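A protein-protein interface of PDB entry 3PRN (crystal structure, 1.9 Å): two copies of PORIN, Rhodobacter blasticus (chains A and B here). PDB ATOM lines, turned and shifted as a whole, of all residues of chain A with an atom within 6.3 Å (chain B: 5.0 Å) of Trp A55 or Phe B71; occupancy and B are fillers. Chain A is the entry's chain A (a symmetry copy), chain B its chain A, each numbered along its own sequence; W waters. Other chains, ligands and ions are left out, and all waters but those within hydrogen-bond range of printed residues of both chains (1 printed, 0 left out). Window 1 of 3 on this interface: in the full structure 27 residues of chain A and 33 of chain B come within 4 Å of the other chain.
O of Asn B67 is in hydrogen-bond range of OG1 of Thr A64 (2.8 Å). The backbone carbonyl oxygen (O) of Ala A62 is in hydrogen-bond range of the backbone NH (N) of Ala B68, 3.3 Å away.
The backbone carbonyl oxygen (O) of Gly B48 lies within hydrogen-bond range of the backbone NH (N) of Trp B72 (2.9 Å). O of Phe B71 sits at hydrogen-bond distance from N of Val B82 (2.8 Å). The backbone NH of Thr B73 is in hydrogen-bond range of the backbone carbonyl oxygen of Val B80. The side-chain hydroxyl of Tyr A7 is in hydrogen-bond range of the guanidinium group of Arg A30, at 3.1 Å. The backbone NH (N) of Arg A30 sits at hydrogen-bond distance from the backbone carbonyl oxygen (O) of Arg A9, 3.0 Å away. The side-chain amide nitrogen (NE2) of Gln A54 sits close to the guanidinium group (NE) of Arg A30, at 3.4 Å.
O of Arg A9 touches CE2 of Phe B71, 3.9 Å away. Thr B73 touches Phe A10 (CG2 to CZ, 3.5 Å). Val B82 touches Phe A10 (CG1 to CG, 3.9 Å). Ser A29 touches Phe B71. O of Arg A30 touches CE2 of Phe B71, 3.3 Å away. Leu A31 touches Ala B49. CB of Ala B69 touches CB of Leu A31, 3.8 Å away. CE1 of Phe B71 touches CZ3 of Trp A55, at 3.9 Å. C of Asn B67 touches O of Ala A62 (3.6 Å). Phe A287 touches Gly B48 (CZ to O, 3.4 Å).
Printed residues of chain A within 4 Å of Phe B71: Arg A9 (3.9 Å), Phe A10 (3.6 Å), Ser A29 (3.5 Å), Arg A30 (3.3 Å) and Trp A55 (3.9 Å). Of the printed residues of chain A, Ala B68 touches Trp A55 (3.7 Å) and Ala A62 (3.3 Å). Of the printed residues of chain B, Ser A29 touches Phe B71. Printed residues of chain B within 4 Å of Phe A287: Gly B48 (3.4 Å). Printed residues of chain B within 4 Å of Thr A64: Asn B67. Of the printed residues of chain A, Thr B73 touches Phe A10. Asp A57 touches none of the printed residues of chain B. Gln A54 touches none of the printed residues of chain B. The nearest residue of chain B that does not touch Trp A55 is Asn B67 (4.3 Å). The nearest printed residue of chain B that does not touch Arg A30 is Ala B69 (5.6 Å).
Hydrophobic or aromatic side chains of chain B that line the printed part of chain A: Ala B49, Ala B68, Ala B69, Phe B71 and Val B82. Of the 20 printed residues of chain A, 10 touch a printed residue of chain B. Hydrophobic or aromatic side chains of chain A within 4 Å of the printed part of chain B: Phe A10, Leu A31, Trp A55 and Phe A287. Along chain A the printed residues that touch a printed residue of chain B span positions 9 to 287. Among the printed residues, 16 pairs touch across the chains.
No position is printed for both chains. Of the 16 pairs that touch across the chains among the printed residues, none has its exchanged pair printed and touching as well.
Water W1 bridges O of Ala A62 (2.8 Å) and N of Ala B68 (3.1 Å).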
ATOM      1  N   TYR A   7     -14.364 -21.640 -29.794  1.00  0.00           N
ATOM      2  CA  TYR A   7     -15.007 -22.528 -30.750  1.00  0.00           C
ATOM      3  C   TYR A   7     -15.508 -23.780 -30.037  1.00  0.00           C
ATOM      4  O   TYR A   7     -15.077 -24.116 -28.931  1.00  0.00           O
ATOM      5  CB  TYR A   7     -14.072 -22.930 -31.881  1.00  0.00           C
ATOM      6  CG  TYR A   7     -12.908 -23.848 -31.622  1.00  0.00           C
ATOM      7  CD1 TYR A   7     -13.094 -25.201 -31.383  1.00  0.00           C
ATOM      8  CD2 TYR A   7     -11.614 -23.328 -31.625  1.00  0.00           C
ATOM      9  CE1 TYR A   7     -11.994 -26.036 -31.146  1.00  0.00           C
ATOM     10  CE2 TYR A   7     -10.499 -24.131 -31.403  1.00  0.00           C
ATOM     11  CZ  TYR A   7     -10.706 -25.480 -31.167  1.00  0.00           C
ATOM     12  OH  TYR A   7      -9.618 -26.306 -30.955  1.00  0.00           O
ATOM     13  N   GLY A   8     -16.533 -24.391 -30.650  1.00  0.00           N
ATOM     14  CA  GLY A   8     -16.994 -25.675 -30.178  1.00  0.00           C
ATOM     15  C   GLY A   8     -16.840 -26.620 -31.421  1.00  0.00           C
ATOM     16  O   GLY A   8     -16.863 -26.136 -32.564  1.00  0.00           O
ATOM     17  N   ARG A   9     -16.619 -27.893 -31.129  1.00  0.00           N
ATOM     18  CA  ARG A   9     -16.597 -28.884 -32.218  1.00  0.00           C
ATOM     19  C   ARG A   9     -17.131 -30.189 -31.651  1.00  0.00           C
ATOM     20  O   ARG A   9     -16.862 -30.516 -30.478  1.00  0.00           O
ATOM     21  CB  ARG A   9     -15.245 -29.034 -32.883  1.00  0.00           C
ATOM     22  CG  ARG A   9     -14.230 -29.858 -32.079  1.00  0.00           C
ATOM     23  CD  ARG A   9     -12.845 -29.784 -32.738  1.00  0.00           C
ATOM     24  NE  ARG A   9     -11.939 -30.652 -32.028  1.00  0.00           N
ATOM     25  CZ  ARG A   9     -10.595 -30.585 -32.132  1.00  0.00           C
ATOM     26  NH1 ARG A   9     -10.007 -29.708 -32.896  1.00  0.00           N
ATOM     27  NH2 ARG A   9      -9.931 -31.478 -31.402  1.00  0.00           N
ATOM     28  N   PHE A  10     -17.797 -30.963 -32.517  1.00  0.00           N
ATOM     29  CA  PHE A  10     -18.219 -32.308 -32.060  1.00  0.00           C
ATOM     30  C   PHE A  10     -18.388 -33.205 -33.289  1.00  0.00           C
ATOM     31  O   PHE A  10     -18.646 -32.663 -34.382  1.00  0.00           O
ATOM     32  CB  PHE A  10     -19.496 -32.204 -31.205  1.00  0.00           C
ATOM     33  CG  PHE A  10     -20.714 -31.670 -31.908  1.00  0.00           C
ATOM     34  CD1 PHE A  10     -21.470 -32.490 -32.717  1.00  0.00           C
ATOM     35  CD2 PHE A  10     -21.124 -30.351 -31.770  1.00  0.00           C
ATOM     36  CE1 PHE A  10     -22.590 -32.024 -33.399  1.00  0.00           C
ATOM     37  CE2 PHE A  10     -22.267 -29.905 -32.415  1.00  0.00           C
ATOM     38  CZ  PHE A  10     -22.992 -30.717 -33.225  1.00  0.00           C
ATOM     39  N   SER A  29     -15.418 -34.402 -28.731  1.00  0.00           N
ATOM     40  CA  SER A  29     -15.819 -32.993 -28.790  1.00  0.00           C
ATOM     41  C   SER A  29     -14.909 -32.130 -27.945  1.00  0.00           C
ATOM     42  O   SER A  29     -14.171 -32.635 -27.091  1.00  0.00           O
ATOM     43  CB  SER A  29     -17.285 -32.891 -28.322  1.00  0.00           C
ATOM     44  OG  SER A  29     -17.400 -33.365 -27.017  1.00  0.00           O
ATOM     45  N   ARG A  30     -14.948 -30.823 -28.234  1.00  0.00           N
ATOM     46  CA  ARG A  30     -14.039 -29.903 -27.518  1.00  0.00           C
ATOM     47  C   ARG A  30     -14.739 -28.541 -27.396  1.00  0.00           C
ATOM     48  O   ARG A  30     -15.365 -28.087 -28.349  1.00  0.00           O
ATOM     49  CB  ARG A  30     -12.749 -29.732 -28.325  1.00  0.00           C
ATOM     50  CG  ARG A  30     -11.882 -28.546 -27.834  1.00  0.00           C
ATOM     51  CD  ARG A  30     -10.604 -28.399 -28.617  1.00  0.00           C
ATOM     52  NE  ARG A  30      -9.697 -29.512 -28.422  1.00  0.00           N
ATOM     53  CZ  ARG A  30      -8.481 -29.591 -29.007  1.00  0.00           C
ATOM     54  NH1 ARG A  30      -8.021 -28.644 -29.799  1.00  0.00           N
ATOM     55  NH2 ARG A  30      -7.773 -30.677 -28.740  1.00  0.00           N
ATOM     56  N   LEU A  31     -14.598 -27.902 -26.249  1.00  0.00           N
ATOM     57  CA  LEU A  31     -15.056 -26.524 -26.111  1.00  0.00           C
ATOM     58  C   LEU A  31     -13.815 -25.675 -25.770  1.00  0.00           C
ATOM     59  O   LEU A  31     -13.104 -26.051 -24.794  1.00  0.00           O
ATOM     60  CB  LEU A  31     -16.126 -26.384 -25.051  1.00  0.00           C
ATOM     61  CG  LEU A  31     -16.428 -24.928 -24.628  1.00  0.00           C
ATOM     62  CD1 LEU A  31     -16.986 -24.183 -25.827  1.00  0.00           C
ATOM     63  CD2 LEU A  31     -17.446 -24.924 -23.503  1.00  0.00           C
ATOM     64  N   ARG A  32     -13.504 -24.643 -26.543  1.00  0.00           N
ATOM     65  CA  ARG A  32     -12.369 -23.797 -26.216  1.00  0.00           C
ATOM     66  C   ARG A  32     -12.860 -22.343 -26.026  1.00  0.00           C
ATOM     67  O   ARG A  32     -13.534 -21.768 -26.915  1.00  0.00           O
ATOM     68  CB  ARG A  32     -11.277 -23.822 -27.325  1.00  0.00           C
ATOM     69  CG  ARG A  32     -10.151 -22.809 -27.003  1.00  0.00           C
ATOM     70  CD  ARG A  32      -9.149 -22.783 -28.199  1.00  0.00           C
ATOM     71  NE  ARG A  32      -8.312 -23.979 -28.133  1.00  0.00           N
ATOM     72  CZ  ARG A  32      -7.342 -24.306 -28.989  1.00  0.00           C
ATOM     73  NH1 ARG A  32      -7.028 -23.502 -30.025  1.00  0.00           N
ATOM     74  NH2 ARG A  32      -6.661 -25.443 -28.801  1.00  0.00           N
ATOM     75  N   MET A  53      -9.585 -21.652 -21.342  1.00  0.00           N
ATOM     76  CA  MET A  53     -10.385 -22.645 -20.639  1.00  0.00           C
ATOM     77  C   MET A  53     -10.829 -23.619 -21.752  1.00  0.00           C
ATOM     78  O   MET A  53     -11.508 -23.254 -22.694  1.00  0.00           O
ATOM     79  CB  MET A  53     -11.635 -22.083 -19.943  1.00  0.00           C
ATOM     80  CG  MET A  53     -11.170 -21.177 -18.755  1.00  0.00           C
ATOM     81  SD  MET A  53     -12.693 -20.444 -17.986  1.00  0.00           S
ATOM     82  CE  MET A  53     -13.130 -21.860 -16.978  1.00  0.00           C
ATOM     83  N   GLN A  54     -10.237 -24.832 -21.741  1.00  0.00           N
ATOM     84  CA  GLN A  54     -10.560 -25.808 -22.755  1.00  0.00           C
ATOM     85  C   GLN A  54     -10.990 -27.128 -22.121  1.00  0.00           C
ATOM     86  O   GLN A  54     -10.303 -27.578 -21.205  1.00  0.00           O
ATOM     87  CB  GLN A  54      -9.357 -26.084 -23.643  1.00  0.00           C
ATOM     88  CG  GLN A  54      -9.647 -27.043 -24.819  1.00  0.00           C
ATOM     89  CD  GLN A  54      -8.398 -27.136 -25.690  1.00  0.00           C
ATOM     90  OE1 GLN A  54      -7.993 -26.070 -26.222  1.00  0.00           O
ATOM     91  NE2 GLN A  54      -7.805 -28.309 -25.833  1.00  0.00           N
ATOM     92  N   TRP A  55     -12.076 -27.681 -22.640  1.00  0.00           N
ATOM     93  CA  TRP A  55     -12.566 -28.968 -22.194  1.00  0.00           C
ATOM     94  C   TRP A  55     -12.543 -29.918 -23.416  1.00  0.00           C
ATOM     95  O   TRP A  55     -12.931 -29.526 -24.539  1.00  0.00           O
ATOM     96  CB  TRP A  55     -14.037 -28.829 -21.673  1.00  0.00           C
ATOM     97  CG  TRP A  55     -14.611 -30.191 -21.320  1.00  0.00           C
ATOM     98  CD1 TRP A  55     -14.484 -30.861 -20.130  1.00  0.00           C
ATOM     99  CD2 TRP A  55     -15.401 -31.031 -22.182  1.00  0.00           C
ATOM    100  NE1 TRP A  55     -15.150 -32.047 -20.197  1.00  0.00           N
ATOM    101  CE2 TRP A  55     -15.710 -32.203 -21.443  1.00  0.00           C
ATOM    102  CE3 TRP A  55     -15.823 -30.943 -23.508  1.00  0.00           C
ATOM    103  CZ2 TRP A  55     -16.429 -33.267 -21.995  1.00  0.00           C
ATOM    104  CZ3 TRP A  55     -16.559 -31.981 -24.062  1.00  0.00           C
ATOM    105  CH2 TRP A  55     -16.856 -33.158 -23.281  1.00  0.00           C
ATOM    106  N   ASP A  56     -12.114 -31.139 -23.193  1.00  0.00           N
ATOM    107  CA  ASP A  56     -12.171 -32.213 -24.169  1.00  0.00           C
ATOM    108  C   ASP A  56     -12.901 -33.430 -23.590  1.00  0.00           C
ATOM    109  O   ASP A  56     -12.831 -33.701 -22.404  1.00  0.00           O
ATOM    110  CB  ASP A  56     -10.735 -32.644 -24.597  1.00  0.00           C
ATOM    111  CG  ASP A  56     -10.083 -31.548 -25.475  1.00  0.00           C
ATOM    112  OD1 ASP A  56     -10.251 -31.620 -26.693  1.00  0.00           O
ATOM    113  OD2 ASP A  56      -9.383 -30.674 -24.927  1.00  0.00           O
ATOM    114  N   ASP A  57     -13.585 -34.185 -24.448  1.00  0.00           N
ATOM    115  CA  ASP A  57     -14.234 -35.417 -23.971  1.00  0.00           C
ATOM    116  C   ASP A  57     -13.139 -36.294 -23.350  1.00  0.00           C
ATOM    117  O   ASP A  57     -11.990 -36.363 -23.818  1.00  0.00           O
ATOM    118  CB  ASP A  57     -14.994 -36.132 -25.101  1.00  0.00           C
ATOM    119  CG  ASP A  57     -14.003 -36.640 -26.126  1.00  0.00           C
ATOM    120  OD1 ASP A  57     -13.620 -35.842 -27.015  1.00  0.00           O
ATOM    121  OD2 ASP A  57     -13.561 -37.807 -26.013  1.00  0.00           O
ATOM    122  N   GLY A  58     -13.500 -36.929 -22.240  1.00  0.00           N
ATOM    123  CA  GLY A  58     -12.524 -37.792 -21.527  1.00  0.00           C
ATOM    124  C   GLY A  58     -11.767 -37.056 -20.436  1.00  0.00           C
ATOM    125  O   GLY A  58     -11.081 -37.734 -19.643  1.00  0.00           O
ATOM    126  N   ASP A  59     -11.826 -35.687 -20.371  1.00  0.00           N
ATOM    127  CA  ASP A  59     -11.043 -34.961 -19.367  1.00  0.00           C
ATOM    128  C   ASP A  59     -11.393 -35.418 -17.944  1.00  0.00           C
ATOM    129  O   ASP A  59     -12.545 -35.645 -17.547  1.00  0.00           O
ATOM    130  CB  ASP A  59     -11.250 -33.415 -19.349  1.00  0.00           C
ATOM    131  CG  ASP A  59     -10.414 -32.750 -20.432  1.00  0.00           C
ATOM    132  OD1 ASP A  59      -9.615 -33.428 -21.049  1.00  0.00           O
ATOM    133  OD2 ASP A  59     -10.625 -31.534 -20.680  1.00  0.00           O
ATOM    134  N   ALA A  62     -14.464 -34.466 -15.301  1.00  0.00           N
ATOM    135  CA  ALA A  62     -15.625 -33.897 -15.989  1.00  0.00           C
ATOM    136  C   ALA A  62     -15.719 -32.402 -15.638  1.00  0.00           C
ATOM    137  O   ALA A  62     -16.778 -31.838 -15.397  1.00  0.00           O
ATOM    138  CB  ALA A  62     -16.890 -34.705 -15.690  1.00  0.00           C
ATOM    139  N   GLY A  63     -14.570 -31.709 -15.640  1.00  0.00           N
ATOM    140  CA  GLY A  63     -14.498 -30.300 -15.291  1.00  0.00           C
ATOM    141  C   GLY A  63     -13.548 -29.506 -16.213  1.00  0.00           C
ATOM    142  O   GLY A  63     -12.840 -30.100 -17.038  1.00  0.00           O
ATOM    143  N   THR A  64     -13.608 -28.195 -16.067  1.00  0.00           N
ATOM    144  CA  THR A  64     -12.780 -27.344 -16.928  1.00  0.00           C
ATOM    145  C   THR A  64     -12.114 -26.286 -16.032  1.00  0.00           C
ATOM    146  O   THR A  64     -12.826 -25.714 -15.151  1.00  0.00           O
ATOM    147  CB  THR A  64     -13.697 -26.588 -17.927  1.00  0.00           C
ATOM    148  OG1 THR A  64     -14.511 -27.562 -18.613  1.00  0.00           O
ATOM    149  CG2 THR A  64     -12.927 -25.819 -19.026  1.00  0.00           C
ATOM    150  N   LYS A 120      -3.919 -26.425 -21.330  1.00  0.00           N
ATOM    151  CA  LYS A 120      -4.560 -26.816 -20.110  1.00  0.00           C
ATOM    152  C   LYS A 120      -3.600 -26.904 -18.930  1.00  0.00           C
ATOM    153  O   LYS A 120      -2.390 -26.823 -19.181  1.00  0.00           O
ATOM    154  CB  LYS A 120      -5.074 -28.277 -20.288  1.00  0.00           C
ATOM    155  CG  LYS A 120      -6.219 -28.284 -21.316  1.00  0.00           C
ATOM    156  CD  LYS A 120      -6.810 -29.693 -21.343  1.00  0.00           C
ATOM    157  CE  LYS A 120      -7.954 -29.744 -22.329  1.00  0.00           C
ATOM    158  NZ  LYS A 120      -8.473 -31.115 -22.526  1.00  0.00           N
ATOM    159  N   PHE A 287     -17.640 -24.828 -35.051  1.00  0.00           N
ATOM    160  CA  PHE A 287     -18.274 -23.540 -35.164  1.00  0.00           C
ATOM    161  C   PHE A 287     -17.511 -22.543 -34.263  1.00  0.00           C
ATOM    162  O   PHE A 287     -17.193 -22.836 -33.124  1.00  0.00           O
ATOM    163  CB  PHE A 287     -19.752 -23.593 -34.855  1.00  0.00           C
ATOM    164  CG  PHE A 287     -20.120 -24.264 -33.548  1.00  0.00           C
ATOM    165  CD1 PHE A 287     -20.176 -25.637 -33.437  1.00  0.00           C
ATOM    166  CD2 PHE A 287     -20.372 -23.475 -32.433  1.00  0.00           C
ATOM    167  CE1 PHE A 287     -20.590 -26.254 -32.237  1.00  0.00           C
ATOM    168  CE2 PHE A 287     -20.753 -24.076 -31.234  1.00  0.00           C
ATOM    169  CZ  PHE A 287     -20.862 -25.451 -31.145  1.00  0.00           C
ATOM    170  N   GLY B  48     -24.502 -23.865 -30.834  1.00  0.00           N
ATOM    171  CA  GLY B  48     -24.193 -23.293 -29.530  1.00  0.00           C
ATOM    172  C   GLY B  48     -23.392 -24.258 -28.665  1.00  0.00           C
ATOM    173  O   GLY B  48     -23.351 -25.488 -28.832  1.00  0.00           O
ATOM    174  N   ALA B  49     -22.733 -23.660 -27.671  1.00  0.00           N
ATOM    175  CA  ALA B  49     -21.946 -24.424 -26.713  1.00  0.00           C
ATOM    176  C   ALA B  49     -22.158 -23.731 -25.356  1.00  0.00           C
ATOM    177  O   ALA B  49     -22.321 -22.499 -25.331  1.00  0.00           O
ATOM    178  CB  ALA B  49     -20.489 -24.606 -27.048  1.00  0.00           C
ATOM    179  N   ASN B  67     -17.811 -26.956 -15.521  1.00  0.00           N
ATOM    180  CA  ASN B  67     -18.334 -28.324 -15.639  1.00  0.00           C
ATOM    181  C   ASN B  67     -17.937 -28.901 -17.020  1.00  0.00           C
ATOM    182  O   ASN B  67     -17.034 -28.340 -17.692  1.00  0.00           O
ATOM    183  CB  ASN B  67     -19.836 -28.376 -15.399  1.00  0.00           C
ATOM    184  CG  ASN B  67     -20.656 -27.619 -16.396  1.00  0.00           C
ATOM    185  OD1 ASN B  67     -20.098 -26.844 -17.189  1.00  0.00           O
ATOM    186  ND2 ASN B  67     -21.968 -27.768 -16.407  1.00  0.00           N
ATOM    187  N   ALA B  68     -18.607 -29.988 -17.464  1.00  0.00           N
ATOM    188  CA  ALA B  68     -18.282 -30.531 -18.809  1.00  0.00           C
ATOM    189  C   ALA B  68     -19.238 -29.864 -19.801  1.00  0.00           C
ATOM    190  O   ALA B  68     -20.364 -29.432 -19.440  1.00  0.00           O
ATOM    191  CB  ALA B  68     -18.520 -32.043 -18.767  1.00  0.00           C
ATOM    192  N   ALA B  69     -18.788 -29.675 -21.048  1.00  0.00           N
ATOM    193  CA  ALA B  69     -19.501 -28.874 -22.025  1.00  0.00           C
ATOM    194  C   ALA B  69     -20.740 -29.565 -22.588  1.00  0.00           C
ATOM    195  O   ALA B  69     -20.847 -30.797 -22.597  1.00  0.00           O
ATOM    196  CB  ALA B  69     -18.583 -28.643 -23.278  1.00  0.00           C
ATOM    197  N   GLN B  70     -21.627 -28.712 -23.050  1.00  0.00           N
ATOM    198  CA  GLN B  70     -22.846 -29.109 -23.755  1.00  0.00           C
ATOM    199  C   GLN B  70     -22.792 -28.397 -25.128  1.00  0.00           C
ATOM    200  O   GLN B  70     -22.456 -27.190 -25.159  1.00  0.00           O
ATOM    201  CB  GLN B  70     -24.088 -28.685 -22.975  1.00  0.00           C
ATOM    202  CG  GLN B  70     -25.379 -29.069 -23.699  1.00  0.00           C
ATOM    203  CD  GLN B  70     -26.628 -28.454 -23.073  1.00  0.00           C
ATOM    204  OE1 GLN B  70     -27.220 -27.547 -23.653  1.00  0.00           O
ATOM    205  NE2 GLN B  70     -27.070 -28.901 -21.913  1.00  0.00           N
ATOM    206  N   PHE B  71     -23.166 -29.049 -26.217  1.00  0.00           N
ATOM    207  CA  PHE B  71     -23.199 -28.523 -27.550  1.00  0.00           C
ATOM    208  C   PHE B  71     -24.602 -28.737 -28.147  1.00  0.00           C
ATOM    209  O   PHE B  71     -25.223 -29.757 -27.888  1.00  0.00           O
ATOM    210  CB  PHE B  71     -22.202 -29.181 -28.523  1.00  0.00           C
ATOM    211  CG  PHE B  71     -20.810 -29.268 -27.948  1.00  0.00           C
ATOM    212  CD1 PHE B  71     -20.473 -30.313 -27.115  1.00  0.00           C
ATOM    213  CD2 PHE B  71     -19.880 -28.265 -28.198  1.00  0.00           C
ATOM    214  CE1 PHE B  71     -19.195 -30.404 -26.520  1.00  0.00           C
ATOM    215  CE2 PHE B  71     -18.582 -28.383 -27.649  1.00  0.00           C
ATOM    216  CZ  PHE B  71     -18.256 -29.443 -26.808  1.00  0.00           C
ATOM    217  N   TRP B  72     -25.074 -27.807 -28.960  1.00  0.00           N
ATOM    218  CA  TRP B  72     -26.370 -28.033 -29.610  1.00  0.00           C
ATOM    219  C   TRP B  72     -26.393 -27.428 -31.004  1.00  0.00           C
ATOM    220  O   TRP B  72     -25.603 -26.560 -31.358  1.00  0.00           O
ATOM    221  CB  TRP B  72     -27.509 -27.488 -28.775  1.00  0.00           C
ATOM    222  CG  TRP B  72     -27.573 -25.989 -28.673  1.00  0.00           C
ATOM    223  CD1 TRP B  72     -28.188 -25.103 -29.559  1.00  0.00           C
ATOM    224  CD2 TRP B  72     -27.015 -25.178 -27.629  1.00  0.00           C
ATOM    225  NE1 TRP B  72     -28.026 -23.814 -29.118  1.00  0.00           N
ATOM    226  CE2 TRP B  72     -27.310 -23.832 -27.935  1.00  0.00           C
ATOM    227  CE3 TRP B  72     -26.278 -25.485 -26.476  1.00  0.00           C
ATOM    228  CZ2 TRP B  72     -26.917 -22.777 -27.130  1.00  0.00           C
ATOM    229  CZ3 TRP B  72     -25.881 -24.417 -25.672  1.00  0.00           C
ATOM    230  CH2 TRP B  72     -26.199 -23.083 -26.004  1.00  0.00           C
ATOM    231  N   THR B  73     -27.390 -27.913 -31.787  1.00  0.00           N
ATOM    232  CA  THR B  73     -27.673 -27.389 -33.105  1.00  0.00           C
ATOM    233  C   THR B  73     -29.215 -27.275 -33.177  1.00  0.00           C
ATOM    234  O   THR B  73     -29.861 -28.270 -32.752  1.00  0.00           O
ATOM    235  CB  THR B  73     -27.196 -28.257 -34.270  1.00  0.00           C
ATOM    236  OG1 THR B  73     -28.047 -29.413 -34.378  1.00  0.00           O
ATOM    237  CG2 THR B  73     -25.777 -28.756 -34.022  1.00  0.00           C
ATOM    238  N   VAL B  80     -30.940 -30.469 -31.305  1.00  0.00           N
ATOM    239  CA  VAL B  80     -30.202 -31.674 -31.019  1.00  0.00           C
ATOM    240  C   VAL B  80     -29.016 -31.237 -30.140  1.00  0.00           C
ATOM    241  O   VAL B  80     -28.346 -30.272 -30.520  1.00  0.00           O
ATOM    242  CB  VAL B  80     -29.707 -32.391 -32.256  1.00  0.00           C
ATOM    243  CG1 VAL B  80     -28.983 -33.686 -31.872  1.00  0.00           C
ATOM    244  CG2 VAL B  80     -30.856 -32.795 -33.184  1.00  0.00           C
ATOM    245  N   SER B  81     -28.803 -31.870 -29.026  1.00  0.00           N
ATOM    246  CA  SER B  81     -27.743 -31.554 -28.085  1.00  0.00           C
ATOM    247  C   SER B  81     -26.923 -32.785 -27.776  1.00  0.00           C
ATOM    248  O   SER B  81     -27.363 -33.931 -27.836  1.00  0.00           O
ATOM    249  CB  SER B  81     -28.246 -30.835 -26.825  1.00  0.00           C
ATOM    250  OG  SER B  81     -29.195 -31.643 -26.200  1.00  0.00           O
ATOM    251  N   VAL B  82     -25.625 -32.538 -27.517  1.00  0.00           N
ATOM    252  CA  VAL B  82     -24.670 -33.599 -27.260  1.00  0.00           C
ATOM    253  C   VAL B  82     -23.758 -33.253 -26.086  1.00  0.00           C
ATOM    254  O   VAL B  82     -23.506 -32.014 -25.854  1.00  0.00           O
ATOM    255  CB  VAL B  82     -23.823 -33.878 -28.520  1.00  0.00           C
ATOM    256  CG1 VAL B  82     -23.173 -32.635 -29.099  1.00  0.00           C
ATOM    257  CG2 VAL B  82     -22.758 -34.924 -28.270  1.00  0.00           C
HETATM  258  O   HOH W   1     -19.548 -32.008 -15.367  1.00  0.00           O
